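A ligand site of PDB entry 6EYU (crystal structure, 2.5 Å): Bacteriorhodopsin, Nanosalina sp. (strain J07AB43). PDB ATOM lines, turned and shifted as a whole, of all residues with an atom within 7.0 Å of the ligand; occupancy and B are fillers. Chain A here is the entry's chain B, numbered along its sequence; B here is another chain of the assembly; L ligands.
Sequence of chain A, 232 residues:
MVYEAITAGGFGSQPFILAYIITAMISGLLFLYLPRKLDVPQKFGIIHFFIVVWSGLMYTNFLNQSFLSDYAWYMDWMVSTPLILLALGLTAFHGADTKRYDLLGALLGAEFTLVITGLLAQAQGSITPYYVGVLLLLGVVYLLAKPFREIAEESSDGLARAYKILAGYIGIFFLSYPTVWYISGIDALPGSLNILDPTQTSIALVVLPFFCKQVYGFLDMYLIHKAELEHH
NE2 of Gln 42 of chain B lies within hydrogen-bond range of O2 of the ligand (3.2 Å). O1 of the ligand sits at hydrogen-bond distance from OH of Tyr 142, at 3.5 Å. An oxygen (O4) of the ligand is in hydrogen-bond range of the side-chain carboxylate of Glu 150 (3.4 Å).
The backbone carbonyl oxygen (O) of Leu 143 is in hydrogen-bond range of the backbone NH (N) of Phe 148, 3.3 Å away.
Merely in contact with the ligand: Pro 147 (3.3 Å), Arg 100 (3.4 Å), Leu 143 (3.6 Å), Ala 110 (3.6 Å) and Gly 139 (3.7 Å).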
ATOM      1  N   ARG A 100     -17.473   2.096   4.685  1.00  0.00           N
ATOM      2  CA  ARG A 100     -18.916   2.302   4.779  1.00  0.00           C
ATOM      3  C   ARG A 100     -19.337   3.551   4.015  1.00  0.00           C
ATOM      4  O   ARG A 100     -19.292   4.663   4.550  1.00  0.00           O
ATOM      5  CB  ARG A 100     -19.337   2.411   6.248  1.00  0.00           C
ATOM      6  CG  ARG A 100     -19.444   1.084   6.971  1.00  0.00           C
ATOM      7  CD  ARG A 100     -20.744   0.364   6.642  1.00  0.00           C
ATOM      8  NE  ARG A 100     -21.480  -0.002   7.839  1.00  0.00           N
ATOM      9  CZ  ARG A 100     -22.626   0.553   8.213  1.00  0.00           C
ATOM     10  NH1 ARG A 100     -23.231   0.155   9.330  1.00  0.00           N
ATOM     11  NH2 ARG A 100     -23.198   1.480   7.451  1.00  0.00           N
ATOM     12  N   LEU A 103     -22.483   5.444   5.060  1.00  0.00           N
ATOM     13  CA  LEU A 103     -22.193   6.353   6.159  1.00  0.00           C
ATOM     14  C   LEU A 103     -21.559   7.649   5.653  1.00  0.00           C
ATOM     15  O   LEU A 103     -21.838   8.725   6.167  1.00  0.00           O
ATOM     16  CB  LEU A 103     -21.268   5.688   7.187  1.00  0.00           C
ATOM     17  CG  LEU A 103     -21.956   4.717   8.147  1.00  0.00           C
ATOM     18  CD1 LEU A 103     -20.992   4.293   9.248  1.00  0.00           C
ATOM     19  CD2 LEU A 103     -23.220   5.324   8.734  1.00  0.00           C
ATOM     20  N   ALA A 106     -24.566   9.552   4.438  1.00  0.00           N
ATOM     21  CA  ALA A 106     -25.251  10.125   5.592  1.00  0.00           C
ATOM     22  C   ALA A 106     -24.488  11.333   6.121  1.00  0.00           C
ATOM     23  O   ALA A 106     -25.067  12.396   6.356  1.00  0.00           O
ATOM     24  CB  ALA A 106     -25.393   9.076   6.689  1.00  0.00           C
ATOM     25  N   LEU A 107     -23.187  11.168   6.307  1.00  0.00           N
ATOM     26  CA  LEU A 107     -22.327  12.264   6.743  1.00  0.00           C
ATOM     27  C   LEU A 107     -22.535  13.488   5.858  1.00  0.00           C
ATOM     28  O   LEU A 107     -22.937  14.541   6.332  1.00  0.00           O
ATOM     29  CB  LEU A 107     -20.859  11.835   6.690  1.00  0.00           C
ATOM     30  CG  LEU A 107     -19.879  12.784   7.402  1.00  0.00           C
ATOM     31  CD1 LEU A 107     -20.119  12.764   8.906  1.00  0.00           C
ATOM     32  CD2 LEU A 107     -18.445  12.407   7.080  1.00  0.00           C
ATOM     33  N   GLY A 109     -24.771  14.034   3.452  1.00  0.00           N
ATOM     34  CA  GLY A 109     -26.172  14.413   3.310  1.00  0.00           C
ATOM     35  C   GLY A 109     -26.637  15.293   4.463  1.00  0.00           C
ATOM     36  O   GLY A 109     -27.339  16.274   4.251  1.00  0.00           O
ATOM     37  N   ALA A 110     -26.231  14.937   5.671  1.00  0.00           N
ATOM     38  CA  ALA A 110     -26.614  15.680   6.861  1.00  0.00           C
ATOM     39  C   ALA A 110     -26.107  17.116   6.787  1.00  0.00           C
ATOM     40  O   ALA A 110     -26.829  18.063   7.091  1.00  0.00           O
ATOM     41  CB  ALA A 110     -26.092  14.997   8.117  1.00  0.00           C
ATOM     42  N   GLU A 111     -24.852  17.274   6.368  1.00  0.00           N
ATOM     43  CA  GLU A 111     -24.242  18.587   6.276  1.00  0.00           C
ATOM     44  C   GLU A 111     -25.008  19.475   5.302  1.00  0.00           C
ATOM     45  O   GLU A 111     -25.325  20.621   5.617  1.00  0.00           O
ATOM     46  CB  GLU A 111     -22.781  18.477   5.828  1.00  0.00           C
ATOM     47  CG  GLU A 111     -21.782  18.627   6.968  1.00  0.00           C
ATOM     48  CD  GLU A 111     -21.791  20.018   7.569  1.00  0.00           C
ATOM     49  OE1 GLU A 111     -21.724  20.999   6.813  1.00  0.00           O
ATOM     50  OE2 GLU A 111     -21.888  20.125   8.817  1.00  0.00           O
ATOM     51  N   LEU A 135     -29.705  19.708  15.379  1.00  0.00           N
ATOM     52  CA  LEU A 135     -29.870  18.278  15.610  1.00  0.00           C
ATOM     53  C   LEU A 135     -29.091  17.474  14.569  1.00  0.00           C
ATOM     54  O   LEU A 135     -28.389  16.520  14.918  1.00  0.00           O
ATOM     55  CB  LEU A 135     -31.354  17.897  15.563  1.00  0.00           C
ATOM     56  CG  LEU A 135     -32.007  17.649  16.925  1.00  0.00           C
ATOM     57  CD1 LEU A 135     -31.317  18.448  18.015  1.00  0.00           C
ATOM     58  CD2 LEU A 135     -33.489  17.974  16.877  1.00  0.00           C
ATOM     59  N   LEU A 136     -29.109  17.941  13.329  1.00  0.00           N
ATOM     60  CA  LEU A 136     -28.346  17.291  12.265  1.00  0.00           C
ATOM     61  C   LEU A 136     -26.840  17.422  12.512  1.00  0.00           C
ATOM     62  O   LEU A 136     -26.088  16.472  12.265  1.00  0.00           O
ATOM     63  CB  LEU A 136     -28.691  17.915  10.910  1.00  0.00           C
ATOM     64  CG  LEU A 136     -30.074  17.559  10.363  1.00  0.00           C
ATOM     65  CD1 LEU A 136     -30.414  18.431   9.159  1.00  0.00           C
ATOM     66  CD2 LEU A 136     -30.162  16.082  10.011  1.00  0.00           C
ATOM     67  N   LEU A 137     -26.413  18.585  12.980  1.00  0.00           N
ATOM     68  CA  LEU A 137     -25.007  18.805  13.305  1.00  0.00           C
ATOM     69  C   LEU A 137     -24.529  17.758  14.305  1.00  0.00           C
ATOM     70  O   LEU A 137     -23.436  17.200  14.172  1.00  0.00           O
ATOM     71  CB  LEU A 137     -24.796  20.206  13.879  1.00  0.00           C
ATOM     72  CG  LEU A 137     -23.335  20.582  14.138  1.00  0.00           C
ATOM     73  CD1 LEU A 137     -22.429  19.980  13.080  1.00  0.00           C
ATOM     74  CD2 LEU A 137     -23.166  22.091  14.195  1.00  0.00           C
ATOM     75  N   LEU A 138     -25.357  17.474  15.307  1.00  0.00           N
ATOM     76  CA  LEU A 138     -25.000  16.537  16.365  1.00  0.00           C
ATOM     77  C   LEU A 138     -24.926  15.114  15.821  1.00  0.00           C
ATOM     78  O   LEU A 138     -24.113  14.313  16.268  1.00  0.00           O
ATOM     79  CB  LEU A 138     -26.020  16.603  17.504  1.00  0.00           C
ATOM     80  CG  LEU A 138     -26.242  17.995  18.112  1.00  0.00           C
ATOM     81  CD1 LEU A 138     -27.363  17.951  19.133  1.00  0.00           C
ATOM     82  CD2 LEU A 138     -24.962  18.524  18.733  1.00  0.00           C
ATOM     83  N   GLY A 139     -25.798  14.809  14.857  1.00  0.00           N
ATOM     84  CA  GLY A 139     -25.712  13.552  14.123  1.00  0.00           C
ATOM     85  C   GLY A 139     -24.412  13.437  13.346  1.00  0.00           C
ATOM     86  O   GLY A 139     -23.840  12.353  13.233  1.00  0.00           O
ATOM     87  N   VAL A 140     -23.925  14.576  12.852  1.00  0.00           N
ATOM     88  CA  VAL A 140     -22.678  14.594  12.097  1.00  0.00           C
ATOM     89  C   VAL A 140     -21.491  14.294  13.015  1.00  0.00           C
ATOM     90  O   VAL A 140     -20.670  13.430  12.707  1.00  0.00           O
ATOM     91  CB  VAL A 140     -22.445  15.968  11.427  1.00  0.00           C
ATOM     92  CG1 VAL A 140     -20.974  16.160  11.109  1.00  0.00           C
ATOM     93  CG2 VAL A 140     -23.291  16.083  10.159  1.00  0.00           C
ATOM     94  N   TYR A 142     -21.553  12.914  15.915  1.00  0.00           N
ATOM     95  CA  TYR A 142     -21.728  11.538  16.366  1.00  0.00           C
ATOM     96  C   TYR A 142     -21.149  10.568  15.347  1.00  0.00           C
ATOM     97  O   TYR A 142     -20.391   9.668  15.692  1.00  0.00           O
ATOM     98  CB  TYR A 142     -23.205  11.214  16.601  1.00  0.00           C
ATOM     99  CG  TYR A 142     -23.501   9.728  16.626  1.00  0.00           C
ATOM    100  CD1 TYR A 142     -23.228   8.972  17.754  1.00  0.00           C
ATOM    101  CD2 TYR A 142     -23.875   9.060  15.466  1.00  0.00           C
ATOM    102  CE1 TYR A 142     -23.422   7.601  17.760  1.00  0.00           C
ATOM    103  CE2 TYR A 142     -24.078   7.695  15.463  1.00  0.00           C
ATOM    104  CZ  TYR A 142     -23.863   6.973  16.614  1.00  0.00           C
ATOM    105  OH  TYR A 142     -24.060   5.611  16.619  1.00  0.00           O
ATOM    106  N   LEU A 143     -21.615  10.679  14.107  1.00  0.00           N
ATOM    107  CA  LEU A 143     -21.075   9.890  13.009  1.00  0.00           C
ATOM    108  C   LEU A 143     -19.552   9.908  13.054  1.00  0.00           C
ATOM    109  O   LEU A 143     -18.904   8.870  12.976  1.00  0.00           O
ATOM    110  CB  LEU A 143     -21.562  10.437  11.670  1.00  0.00           C
ATOM    111  CG  LEU A 143     -22.349   9.481  10.782  1.00  0.00           C
ATOM    112  CD1 LEU A 143     -23.017   8.393  11.613  1.00  0.00           C
ATOM    113  CD2 LEU A 143     -23.373  10.249   9.961  1.00  0.00           C
ATOM    114  N   LYS A 146     -17.870   8.220  16.265  1.00  0.00           N
ATOM    115  CA  LYS A 146     -17.975   6.785  16.523  1.00  0.00           C
ATOM    116  C   LYS A 146     -17.697   5.948  15.272  1.00  0.00           C
ATOM    117  O   LYS A 146     -16.595   5.413  15.126  1.00  0.00           O
ATOM    118  CB  LYS A 146     -19.343   6.437  17.106  1.00  0.00           C
ATOM    119  CG  LYS A 146     -19.268   5.839  18.506  1.00  0.00           C
ATOM    120  CD  LYS A 146     -19.615   6.865  19.571  1.00  0.00           C
ATOM    121  N   PRO A 147     -18.725   5.726  14.447  1.00  0.00           N
ATOM    122  CA  PRO A 147     -18.558   4.766  13.358  1.00  0.00           C
ATOM    123  C   PRO A 147     -17.279   5.019  12.557  1.00  0.00           C
ATOM    124  O   PRO A 147     -16.560   4.077  12.216  1.00  0.00           O
ATOM    125  CB  PRO A 147     -19.792   4.996  12.468  1.00  0.00           C
ATOM    126  CG  PRO A 147     -20.770   5.720  13.341  1.00  0.00           C
ATOM    127  CD  PRO A 147     -19.940   6.537  14.278  1.00  0.00           C
ATOM    128  N   PHE A 148     -17.067   6.277  12.176  1.00  0.00           N
ATOM    129  CA  PHE A 148     -15.924   6.636  11.359  1.00  0.00           C
ATOM    130  C   PHE A 148     -14.625   6.497  12.150  1.00  0.00           C
ATOM    131  O   PHE A 148     -13.603   6.089  11.601  1.00  0.00           O
ATOM    132  CB  PHE A 148     -16.063   8.073  10.856  1.00  0.00           C
ATOM    133  CG  PHE A 148     -16.810   8.192   9.550  1.00  0.00           C
ATOM    134  CD1 PHE A 148     -16.208   7.810   8.365  1.00  0.00           C
ATOM    135  CD2 PHE A 148     -18.152   8.536   9.545  1.00  0.00           C
ATOM    136  CE1 PHE A 148     -16.910   7.863   7.179  1.00  0.00           C
ATOM    137  CE2 PHE A 148     -18.854   8.589   8.359  1.00  0.00           C
ATOM    138  CZ  PHE A 148     -18.234   8.257   7.168  1.00  0.00           C
ATOM    139  N   GLU A 150     -14.255   4.199  14.520  1.00  0.00           N
ATOM    140  CA  GLU A 150     -14.088   2.757  14.516  1.00  0.00           C
ATOM    141  C   GLU A 150     -13.326   2.314  13.279  1.00  0.00           C
ATOM    142  O   GLU A 150     -12.413   1.488  13.342  1.00  0.00           O
ATOM    143  CB  GLU A 150     -15.447   2.058  14.571  1.00  0.00           C
ATOM    144  CG  GLU A 150     -15.574   1.015  15.656  1.00  0.00           C
ATOM    145  CD  GLU A 150     -16.875   0.246  15.566  1.00  0.00           C
ATOM    146  OE1 GLU A 150     -17.955   0.878  15.626  1.00  0.00           O
ATOM    147  OE2 GLU A 150     -16.825  -0.987  15.336  1.00  0.00           O
ATOM    148  N   LEU B  32     -34.324   6.251  11.853  1.00  0.00           N
ATOM    149  CA  LEU B  32     -32.939   6.085  12.295  1.00  0.00           C
ATOM    150  C   LEU B  32     -32.834   4.954  13.308  1.00  0.00           C
ATOM    151  O   LEU B  32     -31.928   4.131  13.240  1.00  0.00           O
ATOM    152  CB  LEU B  32     -32.416   7.392  12.922  1.00  0.00           C
ATOM    153  CG  LEU B  32     -32.000   8.478  11.939  1.00  0.00           C
ATOM    154  CD1 LEU B  32     -31.291   9.613  12.675  1.00  0.00           C
ATOM    155  CD2 LEU B  32     -31.103   7.912  10.849  1.00  0.00           C
ATOM    156  N   GLN B  42     -28.649  -0.473   7.408  1.00  0.00           N
ATOM    157  CA  GLN B  42     -28.812   0.878   7.921  1.00  0.00           C
ATOM    158  C   GLN B  42     -29.164   1.853   6.798  1.00  0.00           C
ATOM    159  O   GLN B  42     -29.846   2.850   7.022  1.00  0.00           O
ATOM    160  CB  GLN B  42     -27.525   1.342   8.611  1.00  0.00           C
ATOM    161  CG  GLN B  42     -27.454   0.957  10.083  1.00  0.00           C
ATOM    162  CD  GLN B  42     -28.213   1.925  10.978  1.00  0.00           C
ATOM    163  OE1 GLN B  42     -29.097   2.641  10.520  1.00  0.00           O
ATOM    164  NE2 GLN B  42     -27.826   1.970  12.248  1.00  0.00           N
ATOM    165  N   ILE B  46     -31.469   5.293   6.997  1.00  0.00           N
ATOM    166  CA  ILE B  46     -30.838   6.578   6.694  1.00  0.00           C
ATOM    167  C   ILE B  46     -31.581   7.284   5.564  1.00  0.00           C
ATOM    168  O   ILE B  46     -31.892   8.472   5.663  1.00  0.00           O
ATOM    169  CB  ILE B  46     -29.367   6.378   6.273  1.00  0.00           C
ATOM    170  CG1 ILE B  46     -28.508   6.069   7.507  1.00  0.00           C
ATOM    171  CG2 ILE B  46     -28.848   7.615   5.566  1.00  0.00           C
ATOM    172  CD1 ILE B  46     -27.184   5.407   7.173  1.00  0.00           C
ATOM    173  N   PHE B  49     -34.970   8.542   6.487  1.00  0.00           N
ATOM    174  CA  PHE B  49     -34.762   9.686   7.366  1.00  0.00           C
ATOM    175  C   PHE B  49     -34.685  10.979   6.551  1.00  0.00           C
ATOM    176  O   PHE B  49     -35.347  11.963   6.866  1.00  0.00           O
ATOM    177  CB  PHE B  49     -33.483   9.509   8.183  1.00  0.00           C
ATOM    178  CG  PHE B  49     -33.004  10.771   8.854  1.00  0.00           C
ATOM    179  CD1 PHE B  49     -33.462  11.112  10.113  1.00  0.00           C
ATOM    180  CD2 PHE B  49     -32.013  11.541   8.273  1.00  0.00           C
ATOM    181  CE1 PHE B  49     -32.980  12.231  10.760  1.00  0.00           C
ATOM    182  CE2 PHE B  49     -31.543  12.675   8.909  1.00  0.00           C
ATOM    183  CZ  PHE B  49     -32.022  13.017  10.158  1.00  0.00           C
ATOM    184  N   PHE B  50     -33.883  10.952   5.482  1.00  0.00           N
ATOM    185  CA  PHE B  50     -33.623  12.151   4.701  1.00  0.00           C
ATOM    186  C   PHE B  50     -34.821  12.506   3.829  1.00  0.00           C
ATOM    187  O   PHE B  50     -35.200  13.675   3.719  1.00  0.00           O
ATOM    188  CB  PHE B  50     -32.386  11.954   3.820  1.00  0.00           C
ATOM    189  CG  PHE B  50     -31.094  12.248   4.531  1.00  0.00           C
ATOM    190  CD1 PHE B  50     -30.825  13.521   5.006  1.00  0.00           C
ATOM    191  CD2 PHE B  50     -30.214  11.230   4.832  1.00  0.00           C
ATOM    192  CE1 PHE B  50     -29.676  13.780   5.732  1.00  0.00           C
ATOM    193  CE2 PHE B  50     -29.061  11.480   5.559  1.00  0.00           C
ATOM    194  CZ  PHE B  50     -28.795  12.749   6.012  1.00  0.00           C
HETATM  195  C1  LIG L   1     -27.451  12.933  10.796  1.00  0.00           C
HETATM  196  C2  LIG L   1     -27.402  11.579  11.494  1.00  0.00           C
HETATM  197  C3  LIG L   1     -27.795  10.478  10.504  1.00  0.00           C
HETATM  198  C4  LIG L   1     -27.171   9.155  10.951  1.00  0.00           C
HETATM  199  C5  LIG L   1     -27.148   9.094  12.481  1.00  0.00           C
HETATM  200  C6  LIG L   1     -27.339   7.646  12.931  1.00  0.00           C
HETATM  201  C7  LIG L   1     -26.865   6.710  11.817  1.00  0.00           C
HETATM  202  C8  LIG L   1     -25.589   5.978  12.263  1.00  0.00           C
HETATM  203  C9  LIG L   1     -25.626   4.449  12.133  1.00  0.00           C
HETATM  204  C10 LIG L   1     -24.609   3.633  12.940  1.00  0.00           C
HETATM  205  O1  LIG L   1     -23.655   4.184  13.493  1.00  0.00           O
HETATM  206  O2  LIG L   1     -24.662   2.292  12.713  1.00  0.00           O
HETATM  207  C11 LIG L   1     -23.386   1.826  12.276  1.00  0.00           C
HETATM  208  C12 LIG L   1     -22.668   1.147  13.436  1.00  0.00           C
HETATM  209  O3  LIG L   1     -21.523   0.447  12.943  1.00  0.00           O
HETATM  210  C13 LIG L   1     -22.213   2.200  14.455  1.00  0.00           C
HETATM  211  O4  LIG L   1     -21.286   1.620  15.365  1.00  0.00           O
